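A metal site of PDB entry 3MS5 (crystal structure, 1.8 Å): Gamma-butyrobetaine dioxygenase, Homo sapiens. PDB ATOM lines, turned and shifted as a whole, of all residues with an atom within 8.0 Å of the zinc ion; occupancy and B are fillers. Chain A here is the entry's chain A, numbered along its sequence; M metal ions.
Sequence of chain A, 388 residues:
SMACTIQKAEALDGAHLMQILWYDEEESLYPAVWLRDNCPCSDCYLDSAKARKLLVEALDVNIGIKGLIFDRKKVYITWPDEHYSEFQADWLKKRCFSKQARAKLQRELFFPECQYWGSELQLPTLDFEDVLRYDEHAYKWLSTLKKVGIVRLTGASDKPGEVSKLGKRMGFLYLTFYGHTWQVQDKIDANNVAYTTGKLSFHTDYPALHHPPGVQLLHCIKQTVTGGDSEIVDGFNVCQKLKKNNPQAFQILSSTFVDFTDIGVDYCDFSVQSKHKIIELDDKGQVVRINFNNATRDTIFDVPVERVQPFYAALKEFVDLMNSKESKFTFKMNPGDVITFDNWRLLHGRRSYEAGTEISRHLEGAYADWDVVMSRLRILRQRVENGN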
ATOM      1  N   LEU A  35      17.653  10.898  -3.857  1.00  0.00           N
ATOM      2  CA  LEU A  35      18.994  11.464  -3.974  1.00  0.00           C
ATOM      3  C   LEU A  35      18.915  13.005  -3.901  1.00  0.00           C
ATOM      4  O   LEU A  35      19.665  13.626  -3.169  1.00  0.00           O
ATOM      5  CB  LEU A  35      19.655  10.991  -5.314  1.00  0.00           C
ATOM      6  CG  LEU A  35      20.015   9.513  -5.426  1.00  0.00           C
ATOM      7  CD1 LEU A  35      20.263   9.121  -6.940  1.00  0.00           C
ATOM      8  CD2 LEU A  35      21.314   9.235  -4.631  1.00  0.00           C
ATOM      9  N   ARG A  36      17.988  13.617  -4.611  1.00  0.00           N
ATOM     10  CA  ARG A  36      17.882  15.075  -4.652  1.00  0.00           C
ATOM     11  C   ARG A  36      17.526  15.597  -3.266  1.00  0.00           C
ATOM     12  O   ARG A  36      18.131  16.546  -2.794  1.00  0.00           O
ATOM     13  CB  ARG A  36      16.873  15.534  -5.694  1.00  0.00           C
ATOM     14  CG  ARG A  36      16.617  17.038  -5.682  1.00  0.00           C
ATOM     15  CD  ARG A  36      17.875  17.784  -6.199  1.00  0.00           C
ATOM     16  NE  ARG A  36      17.804  19.244  -6.063  1.00  0.00           N
ATOM     17  CZ  ARG A  36      18.144  19.920  -4.951  1.00  0.00           C
ATOM     18  NH1 ARG A  36      18.585  19.255  -3.867  1.00  0.00           N
ATOM     19  NH2 ARG A  36      18.099  21.252  -4.939  1.00  0.00           N
ATOM     20  N   ASP A  37      16.588  14.904  -2.610  1.00  0.00           N
ATOM     21  CA  ASP A  37      16.159  15.252  -1.222  1.00  0.00           C
ATOM     22  C   ASP A  37      17.303  15.183  -0.242  1.00  0.00           C
ATOM     23  O   ASP A  37      17.304  15.883   0.749  1.00  0.00           O
ATOM     24  CB  ASP A  37      15.099  14.236  -0.790  1.00  0.00           C
ATOM     25  CG  ASP A  37      14.552  14.503   0.615  1.00  0.00           C
ATOM     26  OD1 ASP A  37      14.168  15.677   0.862  1.00  0.00           O
ATOM     27  OD2 ASP A  37      14.505  13.529   1.397  1.00  0.00           O
ATOM     28  N   ASN A  38      18.274  14.331  -0.528  1.00  0.00           N
ATOM     29  CA  ASN A  38      19.408  14.120   0.367  1.00  0.00           C
ATOM     30  C   ASN A  38      20.757  14.647  -0.156  1.00  0.00           C
ATOM     31  O   ASN A  38      21.823  14.267   0.336  1.00  0.00           O
ATOM     32  CB  ASN A  38      19.447  12.648   0.725  1.00  0.00           C
ATOM     33  CG  ASN A  38      18.276  12.303   1.622  1.00  0.00           C
ATOM     34  OD1 ASN A  38      18.201  12.902   2.700  1.00  0.00           O
ATOM     35  ND2 ASN A  38      17.346  11.446   1.183  1.00  0.00           N
ATOM     36  N   CYS A  39      20.670  15.596  -1.080  1.00  0.00           N
ATOM     37  CA  CYS A  39      21.876  16.365  -1.496  1.00  0.00           C
ATOM     38  C   CYS A  39      22.655  16.874  -0.262  1.00  0.00           C
ATOM     39  O   CYS A  39      22.037  17.510   0.608  1.00  0.00           O
ATOM     40  CB  CYS A  39      21.452  17.569  -2.342  1.00  0.00           C
ATOM     41  SG  CYS A  39      22.954  18.436  -2.959  1.00  0.00           S
ATOM     42  N   PRO A  40      23.970  16.601  -0.153  1.00  0.00           N
ATOM     43  CA  PRO A  40      24.740  17.072   0.998  1.00  0.00           C
ATOM     44  C   PRO A  40      25.379  18.455   0.858  1.00  0.00           C
ATOM     45  O   PRO A  40      26.168  18.840   1.715  1.00  0.00           O
ATOM     46  CB  PRO A  40      25.783  15.956   1.197  1.00  0.00           C
ATOM     47  CG  PRO A  40      26.064  15.474  -0.175  1.00  0.00           C
ATOM     48  CD  PRO A  40      24.774  15.666  -0.983  1.00  0.00           C
ATOM     49  N   CYS A  41      25.069  19.223  -0.206  1.00  0.00           N
ATOM     50  CA  CYS A  41      25.708  20.497  -0.426  1.00  0.00           C
ATOM     51  C   CYS A  41      25.234  21.508   0.609  1.00  0.00           C
ATOM     52  O   CYS A  41      24.181  21.297   1.245  1.00  0.00           O
ATOM     53  CB  CYS A  41      25.474  21.056  -1.856  1.00  0.00           C
ATOM     54  SG  CYS A  41      23.905  21.954  -2.101  1.00  0.00           S
ATOM     55  N   SER A  42      25.949  22.617   0.717  1.00  0.00           N
ATOM     56  CA  SER A  42      25.647  23.602   1.763  1.00  0.00           C
ATOM     57  C   SER A  42      24.292  24.270   1.603  1.00  0.00           C
ATOM     58  O   SER A  42      23.740  24.736   2.596  1.00  0.00           O
ATOM     59  CB  SER A  42      26.753  24.630   1.944  1.00  0.00           C
ATOM     60  OG  SER A  42      27.024  25.336   0.757  1.00  0.00           O
ATOM     61  N   ASP A  43      23.741  24.323   0.391  1.00  0.00           N
ATOM     62  CA  ASP A  43      22.390  24.882   0.221  1.00  0.00           C
ATOM     63  C   ASP A  43      21.346  23.964   0.809  1.00  0.00           C
ATOM     64  O   ASP A  43      20.319  24.433   1.330  1.00  0.00           O
ATOM     65  CB  ASP A  43      22.019  25.049  -1.248  1.00  0.00           C
ATOM     66  CG  ASP A  43      22.874  26.081  -1.975  1.00  0.00           C
ATOM     67  OD1 ASP A  43      23.679  26.820  -1.401  1.00  0.00           O
ATOM     68  OD2 ASP A  43      22.592  26.205  -3.177  1.00  0.00           O
ATOM     69  N   CYS A  44      21.584  22.654   0.704  1.00  0.00           N
ATOM     70  CA  CYS A  44      20.569  21.641   1.032  1.00  0.00           C
ATOM     71  C   CYS A  44      20.717  21.047   2.401  1.00  0.00           C
ATOM     72  O   CYS A  44      19.804  20.421   2.900  1.00  0.00           O
ATOM     73  CB  CYS A  44      20.629  20.493   0.031  1.00  0.00           C
ATOM     74  SG  CYS A  44      20.291  21.011  -1.653  1.00  0.00           S
ATOM     75  N   TYR A  45      21.897  21.211   2.980  1.00  0.00           N
ATOM     76  CA  TYR A  45      22.314  20.438   4.167  1.00  0.00           C
ATOM     77  C   TYR A  45      23.168  21.282   5.050  1.00  0.00           C
ATOM     78  O   TYR A  45      24.190  21.853   4.597  1.00  0.00           O
ATOM     79  CB  TYR A  45      23.108  19.223   3.710  1.00  0.00           C
ATOM     80  CG  TYR A  45      23.410  18.225   4.772  1.00  0.00           C
ATOM     81  CD1 TYR A  45      22.450  17.282   5.133  1.00  0.00           C
ATOM     82  CD2 TYR A  45      24.623  18.207   5.429  1.00  0.00           C
ATOM     83  CE1 TYR A  45      22.694  16.335   6.110  1.00  0.00           C
ATOM     84  CE2 TYR A  45      24.889  17.275   6.424  1.00  0.00           C
ATOM     85  CZ  TYR A  45      23.916  16.338   6.733  1.00  0.00           C
ATOM     86  OH  TYR A  45      24.138  15.393   7.709  1.00  0.00           O
ATOM     87  N   LEU A  54      16.945  21.659   2.912  1.00  0.00           N
ATOM     88  CA  LEU A  54      16.086  21.582   1.742  1.00  0.00           C
ATOM     89  C   LEU A  54      14.620  21.480   2.188  1.00  0.00           C
ATOM     90  O   LEU A  54      14.317  20.761   3.146  1.00  0.00           O
ATOM     91  CB  LEU A  54      16.442  20.378   0.881  1.00  0.00           C
ATOM     92  CG  LEU A  54      15.783  20.278  -0.496  1.00  0.00           C
ATOM     93  CD1 LEU A  54      16.311  21.332  -1.501  1.00  0.00           C
ATOM     94  CD2 LEU A  54      15.935  18.797  -1.037  1.00  0.00           C
ATOM     95  N   TRP A  79      21.247  17.953 -12.114  1.00  0.00           N
ATOM     96  CA  TRP A  79      19.788  17.942 -12.085  1.00  0.00           C
ATOM     97  C   TRP A  79      19.200  18.878 -13.148  1.00  0.00           C
ATOM     98  O   TRP A  79      19.878  19.762 -13.678  1.00  0.00           O
ATOM     99  CB  TRP A  79      19.253  18.352 -10.678  1.00  0.00           C
ATOM    100  CG  TRP A  79      19.719  17.461  -9.574  1.00  0.00           C
ATOM    101  CD1 TRP A  79      20.637  17.742  -8.603  1.00  0.00           C
ATOM    102  CD2 TRP A  79      19.300  16.121  -9.347  1.00  0.00           C
ATOM    103  NE1 TRP A  79      20.818  16.640  -7.789  1.00  0.00           N
ATOM    104  CE2 TRP A  79      19.987  15.657  -8.212  1.00  0.00           C
ATOM    105  CE3 TRP A  79      18.392  15.290  -9.983  1.00  0.00           C
ATOM    106  CZ2 TRP A  79      19.823  14.363  -7.720  1.00  0.00           C
ATOM    107  CZ3 TRP A  79      18.210  14.007  -9.483  1.00  0.00           C
ATOM    108  CH2 TRP A  79      18.929  13.558  -8.357  1.00  0.00           C
ATOM    109  N   HIS A  83      20.977  22.303 -10.516  1.00  0.00           N
ATOM    110  CA  HIS A  83      21.556  21.962  -9.247  1.00  0.00           C
ATOM    111  C   HIS A  83      22.508  20.779  -9.467  1.00  0.00           C
ATOM    112  O   HIS A  83      22.365  20.026 -10.459  1.00  0.00           O
ATOM    113  CB  HIS A  83      20.445  21.595  -8.264  1.00  0.00           C
ATOM    114  CG  HIS A  83      20.893  21.671  -6.855  1.00  0.00           C
ATOM    115  ND1 HIS A  83      21.006  22.867  -6.179  1.00  0.00           N
ATOM    116  CD2 HIS A  83      21.317  20.696  -6.009  1.00  0.00           C
ATOM    117  CE1 HIS A  83      21.468  22.608  -4.957  1.00  0.00           C
ATOM    118  NE2 HIS A  83      21.676  21.307  -4.845  1.00  0.00           N
ATOM    119  N   TYR A  84      23.475  20.650  -8.557  1.00  0.00           N
ATOM    120  CA  TYR A  84      24.601  19.734  -8.687  1.00  0.00           C
ATOM    121  C   TYR A  84      24.836  19.050  -7.352  1.00  0.00           C
ATOM    122  O   TYR A  84      24.860  19.738  -6.328  1.00  0.00           O
ATOM    123  CB  TYR A  84      25.877  20.544  -9.109  1.00  0.00           C
ATOM    124  CG  TYR A  84      27.133  19.735  -8.987  1.00  0.00           C
ATOM    125  CD1 TYR A  84      27.346  18.656  -9.843  1.00  0.00           C
ATOM    126  CD2 TYR A  84      28.055  19.968  -7.993  1.00  0.00           C
ATOM    127  CE1 TYR A  84      28.450  17.884  -9.763  1.00  0.00           C
ATOM    128  CE2 TYR A  84      29.223  19.172  -7.886  1.00  0.00           C
ATOM    129  CZ  TYR A  84      29.416  18.126  -8.796  1.00  0.00           C
ATOM    130  OH  TYR A  84      30.524  17.293  -8.761  1.00  0.00           O
ATOM    131  N   SER A  85      24.957  17.717  -7.354  1.00  0.00           N
ATOM    132  CA  SER A  85      25.170  16.928  -6.155  1.00  0.00           C
ATOM    133  C   SER A  85      26.310  15.893  -6.260  1.00  0.00           C
ATOM    134  O   SER A  85      26.523  15.302  -7.324  1.00  0.00           O
ATOM    135  CB  SER A  85      23.879  16.188  -5.722  1.00  0.00           C
ATOM    136  OG  SER A  85      22.744  17.050  -5.690  1.00  0.00           O
ATOM    137  N   GLU A  86      26.978  15.651  -5.134  1.00  0.00           N
ATOM    138  CA  GLU A  86      27.991  14.583  -4.978  1.00  0.00           C
ATOM    139  C   GLU A  86      27.610  13.624  -3.830  1.00  0.00           C
ATOM    140  O   GLU A  86      27.236  14.058  -2.731  1.00  0.00           O
ATOM    141  CB  GLU A  86      29.397  15.135  -4.690  1.00  0.00           C
ATOM    142  CG  GLU A  86      29.965  15.964  -5.785  1.00  0.00           C
ATOM    143  CD  GLU A  86      31.381  16.510  -5.516  1.00  0.00           C
ATOM    144  OE1 GLU A  86      31.996  16.190  -4.447  1.00  0.00           O
ATOM    145  OE2 GLU A  86      31.828  17.269  -6.442  1.00  0.00           O
ATOM    146  N   PHE A  87      27.696  12.317  -4.109  1.00  0.00           N
ATOM    147  CA  PHE A  87      27.390  11.269  -3.124  1.00  0.00           C
ATOM    148  C   PHE A  87      28.549  10.316  -3.018  1.00  0.00           C
ATOM    149  O   PHE A  87      29.119   9.875  -4.041  1.00  0.00           O
ATOM    150  CB  PHE A  87      26.123  10.504  -3.505  1.00  0.00           C
ATOM    151  CG  PHE A  87      24.909  11.373  -3.660  1.00  0.00           C
ATOM    152  CD1 PHE A  87      24.127  11.735  -2.561  1.00  0.00           C
ATOM    153  CD2 PHE A  87      24.564  11.837  -4.902  1.00  0.00           C
ATOM    154  CE1 PHE A  87      23.035  12.575  -2.742  1.00  0.00           C
ATOM    155  CE2 PHE A  87      23.494  12.637  -5.106  1.00  0.00           C
ATOM    156  CZ  PHE A  87      22.697  13.015  -4.036  1.00  0.00           C
HETATM  157 ZN    ZN M   1      22.294  20.603  -2.870  1.00  0.00          ZN
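The side-chain hydroxyl (OG) of Ser 85 lies close to the side-chain sulfur (SG) of Cys 39.
The backbone NH (N) of Leu 54 is in hydrogen-bond range of the backbone carbonyl oxygen (O) of Cys 44.
The side-chain sulfur of Cys 44 lies close to the guanidinium group of Arg 36.
The side-chain sulfur of Cys 41 sits close to the backbone NH of Asp 43 (3.4 Å).
Four residues have an atom within 4 Å of the zinc ion: Cys 39, Cys 41, Cys 44 and His 83.
The zinc ion is bound by NE2 of His 83 (2.2 Å), SG of Cys 41 (2.2 Å), SG of Cys 39 (2.3 Å) and SG of Cys 44 (2.4 Å).
The zinc ion has four donor atoms within binding distance.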
